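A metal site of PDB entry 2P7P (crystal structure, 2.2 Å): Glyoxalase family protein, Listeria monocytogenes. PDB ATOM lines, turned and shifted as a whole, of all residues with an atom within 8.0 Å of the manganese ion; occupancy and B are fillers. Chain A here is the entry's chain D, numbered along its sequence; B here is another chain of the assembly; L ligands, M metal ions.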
ATOM      1  N   TYR A  67      -0.249 -24.953 -20.566  1.00  0.00           N
ATOM      2  CA  TYR A  67      -0.753 -24.158 -19.452  1.00  0.00           C
ATOM      3  C   TYR A  67      -1.696 -23.037 -19.907  1.00  0.00           C
ATOM      4  O   TYR A  67      -2.147 -22.233 -19.105  1.00  0.00           O
ATOM      5  CB  TYR A  67       0.440 -23.609 -18.642  1.00  0.00           C
ATOM      6  CG  TYR A  67       0.057 -22.899 -17.361  1.00  0.00           C
ATOM      7  CD1 TYR A  67      -0.816 -23.485 -16.430  1.00  0.00           C
ATOM      8  CD2 TYR A  67       0.558 -21.634 -17.078  1.00  0.00           C
ATOM      9  CE1 TYR A  67      -1.185 -22.812 -15.258  1.00  0.00           C
ATOM     10  CE2 TYR A  67       0.203 -20.961 -15.915  1.00  0.00           C
ATOM     11  CZ  TYR A  67      -0.667 -21.541 -15.013  1.00  0.00           C
ATOM     12  OH  TYR A  67      -1.011 -20.817 -13.890  1.00  0.00           O
ATOM     13  N   ASN A  68      -1.994 -22.984 -21.203  1.00  0.00           N
ATOM     14  CA  ASN A  68      -2.926 -21.985 -21.713  1.00  0.00           C
ATOM     15  C   ASN A  68      -4.218 -22.409 -21.020  1.00  0.00           C
ATOM     16  O   ASN A  68      -4.438 -23.608 -20.835  1.00  0.00           O
ATOM     17  CB  ASN A  68      -3.115 -22.120 -23.232  1.00  0.00           C
ATOM     18  CG  ASN A  68      -1.964 -21.546 -24.040  1.00  0.00           C
ATOM     19  OD1 ASN A  68      -1.865 -20.337 -24.213  1.00  0.00           O
ATOM     20  ND2 ASN A  68      -1.096 -22.425 -24.535  1.00  0.00           N
ATOM     21  N   HIS A  69      -5.058 -21.474 -20.603  1.00  0.00           N
ATOM     22  CA  HIS A  69      -6.291 -21.852 -19.926  1.00  0.00           C
ATOM     23  C   HIS A  69      -7.351 -20.767 -19.764  1.00  0.00           C
ATOM     24  O   HIS A  69      -7.095 -19.576 -19.968  1.00  0.00           O
ATOM     25  CB  HIS A  69      -6.003 -22.486 -18.546  1.00  0.00           C
ATOM     26  CG  HIS A  69      -5.294 -21.577 -17.591  1.00  0.00           C
ATOM     27  ND1 HIS A  69      -3.917 -21.484 -17.536  1.00  0.00           N
ATOM     28  CD2 HIS A  69      -5.756 -20.713 -16.654  1.00  0.00           C
ATOM     29  CE1 HIS A  69      -3.573 -20.614 -16.610  1.00  0.00           C
ATOM     30  NE2 HIS A  69      -4.667 -20.122 -16.060  1.00  0.00           N
ATOM     31  N   ILE A  70      -8.550 -21.203 -19.383  1.00  0.00           N
ATOM     32  CA  ILE A  70      -9.684 -20.321 -19.146  1.00  0.00           C
ATOM     33  C   ILE A  70     -10.107 -20.610 -17.725  1.00  0.00           C
ATOM     34  O   ILE A  70     -10.252 -21.770 -17.341  1.00  0.00           O
ATOM     35  CB  ILE A  70     -10.854 -20.646 -20.092  1.00  0.00           C
ATOM     36  CG1 ILE A  70     -10.419 -20.470 -21.545  1.00  0.00           C
ATOM     37  CG2 ILE A  70     -12.027 -19.756 -19.764  1.00  0.00           C
ATOM     38  CD1 ILE A  70     -11.413 -21.055 -22.570  1.00  0.00           C
ATOM     39  N   ALA A  71     -10.307 -19.558 -16.932  1.00  0.00           N
ATOM     40  CA  ALA A  71     -10.704 -19.747 -15.550  1.00  0.00           C
ATOM     41  C   ALA A  71     -12.029 -19.078 -15.240  1.00  0.00           C
ATOM     42  O   ALA A  71     -12.283 -17.946 -15.643  1.00  0.00           O
ATOM     43  CB  ALA A  71      -9.642 -19.213 -14.611  1.00  0.00           C
ATOM     44  N   PHE A  72     -12.857 -19.803 -14.507  1.00  0.00           N
ATOM     45  CA  PHE A  72     -14.158 -19.307 -14.097  1.00  0.00           C
ATOM     46  C   PHE A  72     -14.089 -18.917 -12.618  1.00  0.00           C
ATOM     47  O   PHE A  72     -13.251 -19.421 -11.860  1.00  0.00           O
ATOM     48  CB  PHE A  72     -15.225 -20.379 -14.348  1.00  0.00           C
ATOM     49  CG  PHE A  72     -15.455 -20.653 -15.807  1.00  0.00           C
ATOM     50  CD1 PHE A  72     -14.693 -21.609 -16.471  1.00  0.00           C
ATOM     51  CD2 PHE A  72     -16.377 -19.915 -16.534  1.00  0.00           C
ATOM     52  CE1 PHE A  72     -14.851 -21.817 -17.849  1.00  0.00           C
ATOM     53  CE2 PHE A  72     -16.548 -20.109 -17.900  1.00  0.00           C
ATOM     54  CZ  PHE A  72     -15.778 -21.060 -18.562  1.00  0.00           C
ATOM     55  N   ARG A  97      -0.417 -25.036  -7.073  1.00  0.00           N
ATOM     56  CA  ARG A  97       0.764 -24.379  -7.615  1.00  0.00           C
ATOM     57  C   ARG A  97       1.395 -23.505  -6.541  1.00  0.00           C
ATOM     58  O   ARG A  97       0.740 -23.139  -5.569  1.00  0.00           O
ATOM     59  CB  ARG A  97       0.381 -23.480  -8.796  1.00  0.00           C
ATOM     60  CG  ARG A  97      -0.262 -24.198  -9.972  1.00  0.00           C
ATOM     61  CD  ARG A  97      -0.634 -23.204 -11.060  1.00  0.00           C
ATOM     62  NE  ARG A  97       0.542 -22.535 -11.620  1.00  0.00           N
ATOM     63  CZ  ARG A  97       1.375 -23.098 -12.494  1.00  0.00           C
ATOM     64  NH1 ARG A  97       1.186 -24.339 -12.909  1.00  0.00           N
ATOM     65  NH2 ARG A  97       2.426 -22.412 -12.938  1.00  0.00           N
ATOM     66  N   SER A 106      -7.084 -21.947  -6.326  1.00  0.00           N
ATOM     67  CA  SER A 106      -7.455 -22.457  -7.641  1.00  0.00           C
ATOM     68  C   SER A 106      -7.511 -23.969  -7.752  1.00  0.00           C
ATOM     69  O   SER A 106      -6.847 -24.698  -7.015  1.00  0.00           O
ATOM     70  CB  SER A 106      -6.472 -21.936  -8.689  1.00  0.00           C
ATOM     71  OG  SER A 106      -6.656 -20.559  -8.955  1.00  0.00           O
ATOM     72  N   ILE A 107      -8.349 -24.441  -8.669  1.00  0.00           N
ATOM     73  CA  ILE A 107      -8.474 -25.856  -8.940  1.00  0.00           C
ATOM     74  C   ILE A 107      -8.154 -25.984 -10.425  1.00  0.00           C
ATOM     75  O   ILE A 107      -8.819 -25.379 -11.269  1.00  0.00           O
ATOM     76  CB  ILE A 107      -9.885 -26.401  -8.713  1.00  0.00           C
ATOM     77  CG1 ILE A 107     -10.360 -26.103  -7.289  1.00  0.00           C
ATOM     78  CG2 ILE A 107      -9.893 -27.904  -8.900  1.00  0.00           C
ATOM     79  CD1 ILE A 107     -11.790 -26.539  -7.041  1.00  0.00           C
ATOM     80  N   TYR A 108      -7.126 -26.757 -10.751  1.00  0.00           N
ATOM     81  CA  TYR A 108      -6.747 -26.930 -12.137  1.00  0.00           C
ATOM     82  C   TYR A 108      -7.097 -28.332 -12.609  1.00  0.00           C
ATOM     83  O   TYR A 108      -6.735 -29.306 -11.969  1.00  0.00           O
ATOM     84  CB  TYR A 108      -5.249 -26.665 -12.323  1.00  0.00           C
ATOM     85  CG  TYR A 108      -4.886 -25.193 -12.450  1.00  0.00           C
ATOM     86  CD1 TYR A 108      -4.443 -24.450 -11.347  1.00  0.00           C
ATOM     87  CD2 TYR A 108      -4.959 -24.561 -13.678  1.00  0.00           C
ATOM     88  CE1 TYR A 108      -4.078 -23.102 -11.479  1.00  0.00           C
ATOM     89  CE2 TYR A 108      -4.610 -23.222 -13.824  1.00  0.00           C
ATOM     90  CZ  TYR A 108      -4.164 -22.500 -12.725  1.00  0.00           C
ATOM     91  OH  TYR A 108      -3.782 -21.193 -12.915  1.00  0.00           O
ATOM     92  N   LEU A 116      -7.206 -26.997 -20.623  1.00  0.00           N
ATOM     93  CA  LEU A 116      -6.994 -26.793 -19.200  1.00  0.00           C
ATOM     94  C   LEU A 116      -8.019 -25.783 -18.691  1.00  0.00           C
ATOM     95  O   LEU A 116      -8.095 -24.645 -19.181  1.00  0.00           O
ATOM     96  CB  LEU A 116      -5.583 -26.270 -18.930  1.00  0.00           C
ATOM     97  CG  LEU A 116      -5.283 -25.959 -17.457  1.00  0.00           C
ATOM     98  CD1 LEU A 116      -5.452 -27.214 -16.623  1.00  0.00           C
ATOM     99  CD2 LEU A 116      -3.859 -25.403 -17.343  1.00  0.00           C
ATOM    100  N   PHE A 117      -8.822 -26.199 -17.719  1.00  0.00           N
ATOM    101  CA  PHE A 117      -9.824 -25.321 -17.123  1.00  0.00           C
ATOM    102  C   PHE A 117      -9.419 -24.964 -15.703  1.00  0.00           C
ATOM    103  O   PHE A 117      -8.614 -25.660 -15.080  1.00  0.00           O
ATOM    104  CB  PHE A 117     -11.203 -25.998 -17.114  1.00  0.00           C
ATOM    105  CG  PHE A 117     -11.894 -25.991 -18.453  1.00  0.00           C
ATOM    106  CD1 PHE A 117     -11.763 -27.056 -19.337  1.00  0.00           C
ATOM    107  CD2 PHE A 117     -12.647 -24.876 -18.852  1.00  0.00           C
ATOM    108  CE1 PHE A 117     -12.371 -27.035 -20.594  1.00  0.00           C
ATOM    109  CE2 PHE A 117     -13.265 -24.838 -20.117  1.00  0.00           C
ATOM    110  CZ  PHE A 117     -13.118 -25.930 -20.984  1.00  0.00           C
ATOM    111  N   GLU A 118      -9.987 -23.880 -15.191  1.00  0.00           N
ATOM    112  CA  GLU A 118      -9.661 -23.457 -13.846  1.00  0.00           C
ATOM    113  C   GLU A 118     -10.845 -22.844 -13.115  1.00  0.00           C
ATOM    114  O   GLU A 118     -11.630 -22.104 -13.686  1.00  0.00           O
ATOM    115  CB  GLU A 118      -8.517 -22.436 -13.886  1.00  0.00           C
ATOM    116  CG  GLU A 118      -7.987 -22.068 -12.504  1.00  0.00           C
ATOM    117  CD  GLU A 118      -7.339 -20.698 -12.474  1.00  0.00           C
ATOM    118  OE1 GLU A 118      -6.503 -20.395 -13.354  1.00  0.00           O
ATOM    119  OE2 GLU A 118      -7.664 -19.918 -11.553  1.00  0.00           O
ATOM    120  N   LEU A 119     -10.960 -23.186 -11.843  1.00  0.00           N
ATOM    121  CA  LEU A 119     -12.005 -22.611 -11.005  1.00  0.00           C
ATOM    122  C   LEU A 119     -11.169 -21.827 -10.004  1.00  0.00           C
ATOM    123  O   LEU A 119     -10.394 -22.404  -9.236  1.00  0.00           O
ATOM    124  CB  LEU A 119     -12.840 -23.685 -10.315  1.00  0.00           C
ATOM    125  CG  LEU A 119     -13.774 -24.508 -11.199  1.00  0.00           C
ATOM    126  CD1 LEU A 119     -14.734 -25.289 -10.316  1.00  0.00           C
ATOM    127  CD2 LEU A 119     -14.547 -23.592 -12.143  1.00  0.00           C
ATOM    128  N   HIS A 120     -11.303 -20.509 -10.041  1.00  0.00           N
ATOM    129  CA  HIS A 120     -10.513 -19.652  -9.172  1.00  0.00           C
ATOM    130  C   HIS A 120     -11.329 -18.861  -8.147  1.00  0.00           C
ATOM    131  O   HIS A 120     -12.321 -18.205  -8.487  1.00  0.00           O
ATOM    132  CB  HIS A 120      -9.702 -18.684 -10.030  1.00  0.00           C
ATOM    133  CG  HIS A 120      -8.862 -17.731  -9.239  1.00  0.00           C
ATOM    134  ND1 HIS A 120      -7.840 -18.146  -8.417  1.00  0.00           N
ATOM    135  CD2 HIS A 120      -8.882 -16.383  -9.158  1.00  0.00           C
ATOM    136  CE1 HIS A 120      -7.266 -17.091  -7.864  1.00  0.00           C
ATOM    137  NE2 HIS A 120      -7.878 -16.003  -8.307  1.00  0.00           N
ATOM    138  N   ARG A 127      -6.009  -9.805  -6.052  1.00  0.00           N
ATOM    139  CA  ARG A 127      -4.675 -10.199  -6.489  1.00  0.00           C
ATOM    140  C   ARG A 127      -3.748  -8.994  -6.572  1.00  0.00           C
ATOM    141  O   ARG A 127      -2.609  -9.036  -6.103  1.00  0.00           O
ATOM    142  CB  ARG A 127      -4.766 -10.895  -7.859  1.00  0.00           C
ATOM    143  CG  ARG A 127      -3.421 -11.242  -8.481  1.00  0.00           C
ATOM    144  CD  ARG A 127      -2.447 -11.797  -7.456  1.00  0.00           C
ATOM    145  NE  ARG A 127      -1.128 -12.070  -8.034  1.00  0.00           N
ATOM    146  CZ  ARG A 127      -0.859 -13.125  -8.791  1.00  0.00           C
ATOM    147  NH1 ARG A 127      -1.821 -14.007  -9.055  1.00  0.00           N
ATOM    148  NH2 ARG A 127       0.353 -13.288  -9.294  1.00  0.00           N
ATOM    149  N   SER B   6     -13.273 -15.475 -14.770  1.00  0.00           N
ATOM    150  CA  SER B   6     -12.276 -14.878 -13.905  1.00  0.00           C
ATOM    151  C   SER B   6     -11.178 -14.296 -14.777  1.00  0.00           C
ATOM    152  O   SER B   6     -10.828 -13.132 -14.661  1.00  0.00           O
ATOM    153  CB  SER B   6     -11.682 -15.923 -12.973  1.00  0.00           C
ATOM    154  OG  SER B   6     -10.553 -15.375 -12.312  1.00  0.00           O
ATOM    155  N   HIS B   7     -10.632 -15.118 -15.668  1.00  0.00           N
ATOM    156  CA  HIS B   7      -9.563 -14.679 -16.571  1.00  0.00           C
ATOM    157  C   HIS B   7      -9.137 -15.763 -17.546  1.00  0.00           C
ATOM    158  O   HIS B   7      -9.468 -16.944 -17.367  1.00  0.00           O
ATOM    159  CB  HIS B   7      -8.338 -14.242 -15.771  1.00  0.00           C
ATOM    160  CG  HIS B   7      -7.747 -15.328 -14.919  1.00  0.00           C
ATOM    161  ND1 HIS B   7      -8.298 -15.715 -13.725  1.00  0.00           N
ATOM    162  CD2 HIS B   7      -6.663 -16.103 -15.108  1.00  0.00           C
ATOM    163  CE1 HIS B   7      -7.571 -16.691 -13.207  1.00  0.00           C
ATOM    164  NE2 HIS B   7      -6.566 -16.947 -14.034  1.00  0.00           N
ATOM    165  N   ILE B   8      -8.397 -15.349 -18.565  1.00  0.00           N
ATOM    166  CA  ILE B   8      -7.861 -16.261 -19.568  1.00  0.00           C
ATOM    167  C   ILE B   8      -6.337 -16.110 -19.518  1.00  0.00           C
ATOM    168  O   ILE B   8      -5.824 -15.000 -19.409  1.00  0.00           O
ATOM    169  CB  ILE B   8      -8.360 -15.902 -20.981  1.00  0.00           C
ATOM    170  CG1 ILE B   8      -9.870 -16.112 -21.072  1.00  0.00           C
ATOM    171  CG2 ILE B   8      -7.664 -16.770 -22.001  1.00  0.00           C
ATOM    172  CD1 ILE B   8     -10.494 -15.602 -22.343  1.00  0.00           C
ATOM    173  N   THR B   9      -5.603 -17.222 -19.591  1.00  0.00           N
ATOM    174  CA  THR B   9      -4.144 -17.165 -19.566  1.00  0.00           C
ATOM    175  C   THR B   9      -3.518 -17.790 -20.809  1.00  0.00           C
ATOM    176  O   THR B   9      -3.765 -18.964 -21.123  1.00  0.00           O
ATOM    177  CB  THR B   9      -3.568 -17.890 -18.344  1.00  0.00           C
ATOM    178  OG1 THR B   9      -3.981 -17.214 -17.155  1.00  0.00           O
ATOM    179  CG2 THR B   9      -2.069 -17.916 -18.405  1.00  0.00           C
ATOM    180  N   PHE B  46      -0.470  -8.781 -16.860  1.00  0.00           N
ATOM    181  CA  PHE B  46      -1.921  -8.846 -16.783  1.00  0.00           C
ATOM    182  C   PHE B  46      -2.430  -7.626 -17.539  1.00  0.00           C
ATOM    183  O   PHE B  46      -1.899  -6.521 -17.379  1.00  0.00           O
ATOM    184  CB  PHE B  46      -2.426  -8.760 -15.344  1.00  0.00           C
ATOM    185  CG  PHE B  46      -2.075  -9.947 -14.492  1.00  0.00           C
ATOM    186  CD1 PHE B  46      -2.366  -9.942 -13.133  1.00  0.00           C
ATOM    187  CD2 PHE B  46      -1.453 -11.061 -15.036  1.00  0.00           C
ATOM    188  CE1 PHE B  46      -2.038 -11.027 -12.334  1.00  0.00           C
ATOM    189  CE2 PHE B  46      -1.111 -12.148 -14.237  1.00  0.00           C
ATOM    190  CZ  PHE B  46      -1.407 -12.133 -12.886  1.00  0.00           C
ATOM    191  N   TRP B  53     -10.068  -9.771 -17.675  1.00  0.00           N
ATOM    192  CA  TRP B  53      -8.746  -9.979 -17.112  1.00  0.00           C
ATOM    193  C   TRP B  53      -7.988 -10.983 -17.991  1.00  0.00           C
ATOM    194  O   TRP B  53      -8.337 -12.170 -18.040  1.00  0.00           O
ATOM    195  CB  TRP B  53      -8.904 -10.475 -15.670  1.00  0.00           C
ATOM    196  CG  TRP B  53      -7.654 -10.838 -14.920  1.00  0.00           C
ATOM    197  CD1 TRP B  53      -6.353 -10.603 -15.293  1.00  0.00           C
ATOM    198  CD2 TRP B  53      -7.582 -11.514 -13.660  1.00  0.00           C
ATOM    199  NE1 TRP B  53      -5.488 -11.101 -14.347  1.00  0.00           N
ATOM    200  CE2 TRP B  53      -6.218 -11.671 -13.328  1.00  0.00           C
ATOM    201  CE3 TRP B  53      -8.547 -12.025 -12.772  1.00  0.00           C
ATOM    202  CZ2 TRP B  53      -5.788 -12.295 -12.160  1.00  0.00           C
ATOM    203  CZ3 TRP B  53      -8.123 -12.641 -11.602  1.00  0.00           C
ATOM    204  CH2 TRP B  53      -6.753 -12.776 -11.307  1.00  0.00           C
ATOM    205  N   CYS B  55      -4.188 -12.656 -18.919  1.00  0.00           N
ATOM    206  CA  CYS B  55      -2.823 -12.884 -18.429  1.00  0.00           C
ATOM    207  C   CYS B  55      -1.964 -13.414 -19.570  1.00  0.00           C
ATOM    208  O   CYS B  55      -2.419 -14.192 -20.405  1.00  0.00           O
ATOM    209  CB  CYS B  55      -3.001 -13.833 -17.246  1.00  0.00           C
ATOM    210  SG  CYS B  55      -4.171 -13.187 -15.974  1.00  0.00           S
HETATM  211  S1  LIG L   1      -2.360 -17.065 -13.695  1.00  0.00           S
HETATM  212  O1  LIG L   1      -1.866 -17.828 -12.540  1.00  0.00           O
HETATM  213  O2  LIG L   1      -1.253 -16.783 -14.608  1.00  0.00           O
HETATM  214  O3  LIG L   1      -3.376 -17.859 -14.418  1.00  0.00           O
HETATM  215  O4  LIG L   1      -2.980 -15.798 -13.243  1.00  0.00           O
HETATM  216 MN    MN M   1      -5.094 -19.045 -13.980  1.00  0.00          MN
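The manganese ion is bound by OE1 of Glu 118 (2.0 Å).
An oxygen (O3) of the ligand is bound to the manganese ion, at 2.1 Å.
The manganese ion is bound by NE2 of His 69 (2.4 Å).
The manganese ion is bound by NE2 of His 7 of chain B (2.6 Å).
The manganese ion has four donor atoms within binding distance.
Slightly farther from the manganese ion lies the side-chain hydroxyl (OH) of Tyr 108 (2.7 Å).
Residues that only touch the manganese ion: Thr 9 of chain B (3.8 Å).
Within 4 Å of the manganese ion: His 69, Tyr 108, Glu 118, His 7 of chain B and Thr 9 of chain B.
The nearest printed residue that does not touch the manganese ion is Tyr 67 (4.5 Å).
OE1 of Glu 118 sits close to OH of Tyr 108, at 2.9 Å.
The side-chain carboxylate of Glu 118 is in hydrogen-bond range of the side-chain hydroxyl of Ser 106.
N of Glu 118 is in hydrogen-bond range of O of Ile 70, at 3.0 Å.
N of Phe 72 sits at hydrogen-bond distance from O of Glu 118 (2.7 Å).
NE2 of His 69 sits close to OH of Tyr 108 (3.4 Å).
N of Thr 9 of chain B is in hydrogen-bond range of O of His 69, at 2.8 Å.
The backbone carbonyl oxygen (O) of His 7 of chain B lies within hydrogen-bond range of the backbone NH (N) of Ala 71 (2.8 Å).
The side-chain hydroxyl of Tyr 67 lies within hydrogen-bond range of the side-chain hydroxyl of Tyr 108 (3.0 Å).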
